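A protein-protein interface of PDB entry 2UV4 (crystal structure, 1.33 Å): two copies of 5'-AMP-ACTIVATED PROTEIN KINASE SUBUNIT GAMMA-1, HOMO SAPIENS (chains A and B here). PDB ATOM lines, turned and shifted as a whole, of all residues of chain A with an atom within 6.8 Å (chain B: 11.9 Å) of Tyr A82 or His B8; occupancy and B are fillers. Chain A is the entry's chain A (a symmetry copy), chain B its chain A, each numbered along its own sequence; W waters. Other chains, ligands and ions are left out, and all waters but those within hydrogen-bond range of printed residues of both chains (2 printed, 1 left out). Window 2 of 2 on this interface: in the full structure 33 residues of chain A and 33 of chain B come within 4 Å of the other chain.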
ATOM      1  N   GLU A  79       0.787 -13.194  30.095  1.00  0.00           N
ATOM      2  CA  GLU A  79       1.430 -14.476  29.754  1.00  0.00           C
ATOM      3  C   GLU A  79       2.311 -14.300  28.538  1.00  0.00           C
ATOM      4  O   GLU A  79       1.886 -13.716  27.562  1.00  0.00           O
ATOM      5  CB  GLU A  79       0.362 -15.526  29.470  1.00  0.00           C
ATOM      6  CG  GLU A  79      -0.404 -15.928  30.721  1.00  0.00           C
ATOM      7  CD  GLU A  79      -1.441 -16.992  30.510  1.00  0.00           C
ATOM      8  OE1 GLU A  79      -1.426 -17.665  29.460  1.00  0.00           O
ATOM      9  OE2 GLU A  79      -2.282 -17.194  31.407  1.00  0.00           O
ATOM     10  N   LYS A  80       3.527 -14.855  28.576  1.00  0.00           N
ATOM     11  CA  LYS A  80       4.459 -14.688  27.456  1.00  0.00           C
ATOM     12  C   LYS A  80       4.107 -15.580  26.273  1.00  0.00           C
ATOM     13  O   LYS A  80       4.481 -15.290  25.148  1.00  0.00           O
ATOM     14  CB  LYS A  80       5.904 -14.890  27.934  1.00  0.00           C
ATOM     15  CG  LYS A  80       6.334 -13.800  28.912  1.00  0.00           C
ATOM     16  CD  LYS A  80       7.788 -13.884  29.334  1.00  0.00           C
ATOM     17  CE  LYS A  80       8.109 -12.791  30.350  1.00  0.00           C
ATOM     18  NZ  LYS A  80       7.892 -11.435  29.769  1.00  0.00           N
ATOM     19  N   THR A  81       3.359 -16.641  26.518  1.00  0.00           N
ATOM     20  CA  THR A  81       2.919 -17.516  25.444  1.00  0.00           C
ATOM     21  C   THR A  81       1.756 -16.877  24.672  1.00  0.00           C
ATOM     22  O   THR A  81       1.098 -15.934  25.172  1.00  0.00           O
ATOM     23  CB  THR A  81       2.495 -18.870  25.988  1.00  0.00           C
ATOM     24  OG1 THR A  81       1.627 -18.669  27.112  1.00  0.00           O
ATOM     25  CG2 THR A  81       3.717 -19.655  26.440  1.00  0.00           C
ATOM     26  N   TYR A  82       1.478 -17.367  23.475  1.00  0.00           N
ATOM     27  CA  TYR A  82       0.486 -16.787  22.601  1.00  0.00           C
ATOM     28  C   TYR A  82      -0.895 -17.196  23.002  1.00  0.00           C
ATOM     29  O   TYR A  82      -1.175 -18.393  23.090  1.00  0.00           O
ATOM     30  CB  TYR A  82       0.756 -17.236  21.163  1.00  0.00           C
ATOM     31  CG  TYR A  82      -0.175 -16.635  20.162  1.00  0.00           C
ATOM     32  CD1 TYR A  82       0.238 -15.560  19.390  1.00  0.00           C
ATOM     33  CD2 TYR A  82      -1.460 -17.107  19.991  1.00  0.00           C
ATOM     34  CE1 TYR A  82      -0.618 -14.980  18.460  1.00  0.00           C
ATOM     35  CE2 TYR A  82      -2.326 -16.547  19.068  1.00  0.00           C
ATOM     36  CZ  TYR A  82      -1.888 -15.472  18.307  1.00  0.00           C
ATOM     37  OH  TYR A  82      -2.750 -14.913  17.399  1.00  0.00           O
ATOM     38  N   ASN A  83      -1.764 -16.219  23.264  1.00  0.00           N
ATOM     39  CA  ASN A  83      -3.159 -16.458  23.528  1.00  0.00           C
ATOM     40  C   ASN A  83      -4.014 -15.591  22.653  1.00  0.00           C
ATOM     41  O   ASN A  83      -3.539 -14.564  22.169  1.00  0.00           O
ATOM     42  CB  ASN A  83      -3.513 -16.112  24.968  1.00  0.00           C
ATOM     43  CG  ASN A  83      -2.798 -16.968  25.971  1.00  0.00           C
ATOM     44  OD1 ASN A  83      -2.976 -18.182  26.006  1.00  0.00           O
ATOM     45  ND2 ASN A  83      -2.016 -16.335  26.836  1.00  0.00           N
ATOM     46  N   ASN A  84      -5.251 -16.015  22.459  1.00  0.00           N
ATOM     47  CA  ASN A  84      -6.306 -15.136  21.941  1.00  0.00           C
ATOM     48  C   ASN A  84      -7.468 -15.167  22.919  1.00  0.00           C
ATOM     49  O   ASN A  84      -7.405 -15.833  23.928  1.00  0.00           O
ATOM     50  CB  ASN A  84      -6.744 -15.566  20.559  1.00  0.00           C
ATOM     51  CG  ASN A  84      -7.189 -16.998  20.493  1.00  0.00           C
ATOM     52  OD1 ASN A  84      -8.010 -17.450  21.278  1.00  0.00           O
ATOM     53  ND2 ASN A  84      -6.636 -17.747  19.518  1.00  0.00           N
ATOM     54  N   LEU A  85      -8.512 -14.395  22.665  1.00  0.00           N
ATOM     55  CA  LEU A  85      -9.575 -14.311  23.671  1.00  0.00           C
ATOM     56  C   LEU A  85     -10.582 -15.425  23.551  1.00  0.00           C
ATOM     57  O   LEU A  85     -11.535 -15.438  24.327  1.00  0.00           O
ATOM     58  CB  LEU A  85     -10.322 -12.990  23.544  1.00  0.00           C
ATOM     59  CG  LEU A  85      -9.649 -11.742  24.031  1.00  0.00           C
ATOM     60  CD1 LEU A  85     -10.412 -10.568  23.476  1.00  0.00           C
ATOM     61  CD2 LEU A  85      -9.635 -11.681  25.577  1.00  0.00           C
ATOM     62  N   ASP A  86     -10.403 -16.347  22.587  1.00  0.00           N
ATOM     63  CA  ASP A  86     -11.272 -17.485  22.493  1.00  0.00           C
ATOM     64  C   ASP A  86     -10.988 -18.545  23.582  1.00  0.00           C
ATOM     65  O   ASP A  86     -11.755 -19.474  23.760  1.00  0.00           O
ATOM     66  CB  ASP A  86     -11.161 -18.097  21.090  1.00  0.00           C
ATOM     67  CG  ASP A  86     -12.418 -18.808  20.653  1.00  0.00           C
ATOM     68  OD1 ASP A  86     -13.419 -18.821  21.378  1.00  0.00           O
ATOM     69  OD2 ASP A  86     -12.396 -19.349  19.529  1.00  0.00           O
ATOM     70  N   LYS A  91      -8.936 -21.143  31.850  1.00  0.00           N
ATOM     71  CA  LYS A  91      -7.473 -21.122  31.794  1.00  0.00           C
ATOM     72  C   LYS A  91      -6.881 -20.385  32.996  1.00  0.00           C
ATOM     73  O   LYS A  91      -5.728 -20.619  33.371  1.00  0.00           O
ATOM     74  CB  LYS A  91      -6.929 -20.536  30.483  1.00  0.00           C
ATOM     75  CG  LYS A  91      -5.621 -21.315  30.090  1.00  0.00           C
ATOM     76  CD  LYS A  91      -5.091 -21.201  28.688  1.00  0.00           C
ATOM     77  CE  LYS A  91      -4.185 -20.030  28.563  1.00  0.00           C
ATOM     78  NZ  LYS A  91      -2.845 -20.126  29.261  1.00  0.00           N
ATOM     79  N   HIS B   8      -5.729 -12.846  15.987  1.00  0.00           N
ATOM     80  CA  HIS B   8      -6.380 -12.013  17.058  1.00  0.00           C
ATOM     81  C   HIS B   8      -5.817 -12.359  18.426  1.00  0.00           C
ATOM     82  O   HIS B   8      -6.559 -12.643  19.363  1.00  0.00           O
ATOM     83  CB  HIS B   8      -7.885 -12.186  17.053  1.00  0.00           C
ATOM     84  CG  HIS B   8      -8.333 -13.601  17.107  1.00  0.00           C
ATOM     85  ND1 HIS B   8      -9.606 -13.963  17.495  1.00  0.00           N
ATOM     86  CD2 HIS B   8      -7.678 -14.752  16.835  1.00  0.00           C
ATOM     87  CE1 HIS B   8      -9.719 -15.277  17.457  1.00  0.00           C
ATOM     88  NE2 HIS B   8      -8.565 -15.780  17.053  1.00  0.00           N
ATOM     89  N   GLU B   9      -4.340 -11.908  18.323  1.00  0.00           N
ATOM     90  CA  GLU B   9      -3.583 -12.132  19.550  1.00  0.00           C
ATOM     91  C   GLU B   9      -4.137 -11.251  20.661  1.00  0.00           C
ATOM     92  O   GLU B   9      -4.527 -10.101  20.411  1.00  0.00           O
ATOM     93  CB  GLU B   9      -2.117 -11.829  19.336  1.00  0.00           C
ATOM     94  CG  GLU B   9      -1.309 -12.153  20.551  1.00  0.00           C
ATOM     95  CD  GLU B   9       0.162 -12.026  20.374  1.00  0.00           C
ATOM     96  OE1 GLU B   9       0.616 -11.708  19.256  1.00  0.00           O
ATOM     97  OE2 GLU B   9       0.875 -12.268  21.356  1.00  0.00           O
ATOM     98  N   PHE B  10      -4.196 -11.805  21.874  1.00  0.00           N
ATOM     99  CA  PHE B  10      -4.553 -11.038  23.059  1.00  0.00           C
ATOM    100  C   PHE B  10      -3.411 -10.955  24.037  1.00  0.00           C
ATOM    101  O   PHE B  10      -2.891 -12.014  24.430  1.00  0.00           O
ATOM    102  CB  PHE B  10      -5.717 -11.667  23.790  1.00  0.00           C
ATOM    103  CG  PHE B  10      -6.098 -10.916  25.024  1.00  0.00           C
ATOM    104  CD1 PHE B  10      -6.741  -9.687  24.911  1.00  0.00           C
ATOM    105  CD2 PHE B  10      -5.820 -11.396  26.279  1.00  0.00           C
ATOM    106  CE1 PHE B  10      -7.084  -8.957  26.060  1.00  0.00           C
ATOM    107  CE2 PHE B  10      -6.133 -10.667  27.404  1.00  0.00           C
ATOM    108  CZ  PHE B  10      -6.783  -9.451  27.277  1.00  0.00           C
ATOM    109  N   PRO B  11      -2.989  -9.739  24.403  1.00  0.00           N
ATOM    110  CA  PRO B  11      -3.477  -8.497  23.816  1.00  0.00           C
ATOM    111  C   PRO B  11      -2.807  -8.255  22.486  1.00  0.00           C
ATOM    112  O   PRO B  11      -1.814  -8.919  22.166  1.00  0.00           O
ATOM    113  CB  PRO B  11      -3.008  -7.412  24.819  1.00  0.00           C
ATOM    114  CG  PRO B  11      -2.496  -8.144  25.939  1.00  0.00           C
ATOM    115  CD  PRO B  11      -1.983  -9.431  25.429  1.00  0.00           C
ATOM    116  N   LYS B  12      -3.277  -7.279  21.709  1.00  0.00           N
ATOM    117  CA  LYS B  12      -2.589  -7.032  20.432  1.00  0.00           C
ATOM    118  C   LYS B  12      -1.226  -6.461  20.696  1.00  0.00           C
ATOM    119  O   LYS B  12      -1.109  -5.574  21.555  1.00  0.00           O
ATOM    120  CB  LYS B  12      -3.361  -6.056  19.541  1.00  0.00           C
ATOM    121  CG  LYS B  12      -4.301  -6.724  18.594  1.00  0.00           C
ATOM    122  CD  LYS B  12      -5.045  -5.694  17.734  1.00  0.00           C
ATOM    123  CE  LYS B  12      -6.526  -5.688  18.032  1.00  0.00           C
ATOM    124  NZ  LYS B  12      -7.143  -6.960  17.559  1.00  0.00           N
ATOM    125  N   PRO B  13      -0.177  -6.942  20.011  1.00  0.00           N
ATOM    126  CA  PRO B  13       1.116  -6.378  20.227  1.00  0.00           C
ATOM    127  C   PRO B  13       1.210  -4.870  20.076  1.00  0.00           C
ATOM    128  O   PRO B  13       1.984  -4.253  20.794  1.00  0.00           O
ATOM    129  CB  PRO B  13       1.999  -7.110  19.207  1.00  0.00           C
ATOM    130  CG  PRO B  13       1.320  -8.431  19.093  1.00  0.00           C
ATOM    131  CD  PRO B  13      -0.101  -8.127  19.121  1.00  0.00           C
ATOM    132  N   GLU B  14       0.447  -4.298  19.152  1.00  0.00           N
ATOM    133  CA  GLU B  14       0.499  -2.854  18.924  1.00  0.00           C
ATOM    134  C   GLU B  14      -0.027  -2.092  20.131  1.00  0.00           C
ATOM    135  O   GLU B  14       0.421  -0.979  20.420  1.00  0.00           O
ATOM    136  CB  GLU B  14      -0.265  -2.473  17.658  1.00  0.00           C
ATOM    137  CG  GLU B  14      -1.655  -3.107  17.508  1.00  0.00           C
ATOM    138  CD  GLU B  14      -1.687  -4.333  16.567  1.00  0.00           C
ATOM    139  OE1 GLU B  14      -2.261  -4.187  15.463  1.00  0.00           O
ATOM    140  OE2 GLU B  14      -1.148  -5.426  16.911  1.00  0.00           O
ATOM    141  N   PHE B  15      -0.934  -2.691  20.871  1.00  0.00           N
ATOM    142  CA  PHE B  15      -1.408  -2.094  22.127  1.00  0.00           C
ATOM    143  C   PHE B  15      -0.339  -2.130  23.184  1.00  0.00           C
ATOM    144  O   PHE B  15      -0.092  -1.151  23.887  1.00  0.00           O
ATOM    145  CB  PHE B  15      -2.625  -2.909  22.593  1.00  0.00           C
ATOM    146  CG  PHE B  15      -3.155  -2.514  23.938  1.00  0.00           C
ATOM    147  CD1 PHE B  15      -4.195  -1.625  24.028  1.00  0.00           C
ATOM    148  CD2 PHE B  15      -2.649  -3.077  25.100  1.00  0.00           C
ATOM    149  CE1 PHE B  15      -4.697  -1.248  25.247  1.00  0.00           C
ATOM    150  CE2 PHE B  15      -3.161  -2.707  26.333  1.00  0.00           C
ATOM    151  CZ  PHE B  15      -4.199  -1.800  26.389  1.00  0.00           C
ATOM    152  N   MET B  16       0.315  -3.264  23.320  1.00  0.00           N
ATOM    153  CA  MET B  16       1.313  -3.466  24.331  1.00  0.00           C
ATOM    154  C   MET B  16       2.495  -2.542  24.161  1.00  0.00           C
ATOM    155  O   MET B  16       3.148  -2.194  25.158  1.00  0.00           O
ATOM    156  CB  MET B  16       1.789  -4.924  24.357  1.00  0.00           C
ATOM    157  CG  MET B  16       0.712  -5.899  24.756  1.00  0.00           C
ATOM    158  SD  MET B  16       0.163  -5.655  26.483  1.00  0.00           S
ATOM    159  CE  MET B  16       1.134  -6.887  27.347  1.00  0.00           C
ATOM    160  N   LEU B 149      -8.394  -2.071  26.274  1.00  0.00           N
ATOM    161  CA  LEU B 149      -8.244  -3.320  25.532  1.00  0.00           C
ATOM    162  C   LEU B 149      -9.425  -3.616  24.611  1.00  0.00           C
ATOM    163  O   LEU B 149      -9.257  -4.338  23.628  1.00  0.00           O
ATOM    164  CB  LEU B 149      -8.029  -4.504  26.496  1.00  0.00           C
ATOM    165  CG  LEU B 149      -6.606  -4.617  27.054  1.00  0.00           C
ATOM    166  CD1 LEU B 149      -6.466  -5.574  28.243  1.00  0.00           C
ATOM    167  CD2 LEU B 149      -5.662  -4.999  25.941  1.00  0.00           C
ATOM    168  N   VAL B 150     -10.600  -3.073  24.892  1.00  0.00           N
ATOM    169  CA  VAL B 150     -11.784  -3.405  24.092  1.00  0.00           C
ATOM    170  C   VAL B 150     -12.008  -2.436  22.934  1.00  0.00           C
ATOM    171  O   VAL B 150     -12.467  -2.865  21.870  1.00  0.00           O
ATOM    172  CB  VAL B 150     -13.043  -3.476  24.960  1.00  0.00           C
ATOM    173  CG1 VAL B 150     -12.833  -4.476  26.078  1.00  0.00           C
ATOM    174  CG2 VAL B 150     -13.394  -2.124  25.523  1.00  0.00           C
HETATM  175  O   HOH W   1      -1.507 -13.437  26.481  1.00  0.00           O
HETATM  176  O   HOH W   2      -8.462 -12.158  20.836  1.00  0.00           O
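The backbone NH of Phe B10 lies within hydrogen-bond range of the backbone carbonyl oxygen of Asn A83, 2.9 Å away.
The side-chain amide nitrogen (ND2) of Asn A83 lies within hydrogen-bond range of the side-chain carboxylate (OE1) of Glu A79, 3.0 Å away.
The side-chain amide oxygen of Asn A84 lies within hydrogen-bond range of the backbone NH of Asp A86, at 2.9 Å.
Of the printed residues of chain B, Tyr A82 touches His B8 (3.9 Å) and Glu B9 (3.5 Å).
Of chain A, only Tyr A82 (3.9 Å) and Asn A84 (3.2 Å) come within 4 Å of His B8.
No residue of chain B comes within 4 Å of Thr A81.
Of the printed residues of chain A, Phe B10 touches Asn A83, Asn A84 and Leu A85.
Printed residues of chain A within 4 Å of Glu B9: Tyr A82 (3.5 Å) and Asn A83 (3.6 Å).
Glu B14 touches none of the printed residues of chain A.
Met B16 touches none of the printed residues of chain A.
The nearest residue of chain B that does not touch Tyr A82 is Phe B10 (5.6 Å).
The nearest residue of chain A that does not touch His B8 is Leu A85 (4.2 Å).
Hydrophobic or aromatic side chains of chain A within 4 Å of the printed part of chain B: Tyr A82 and Leu A85.
Along chain A the printed residues that touch a printed residue of chain B span positions 82 to 85.
Of the 11 printed residues of chain B, 3 touch a printed residue of chain A.
No position is printed for both chains.
Of the 7 pairs that touch across the chains among the printed residues, none has its exchanged pair printed and touching as well.
Water W2 bridges the backbone carbonyl oxygen of His B8 (2.5 Å) and the backbone NH of Leu A85 (2.9 Å).
Water W1 lies within hydrogen-bond range of O of Phe B10 (2.9 Å) and ND2 of Asn A83 (3.0 Å).
Among the printed residues, merely in contact across the chains: Asn A84 with His B8 (3.2 Å), Tyr A82 with Glu B9 (3.5 Å), Asn A83 with Glu B9 (3.6 Å), Leu A85 with Phe B10 (3.6 Å), Tyr A82 with His B8 (3.9 Å) and Asn A84 with Phe B10 (3.9 Å).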
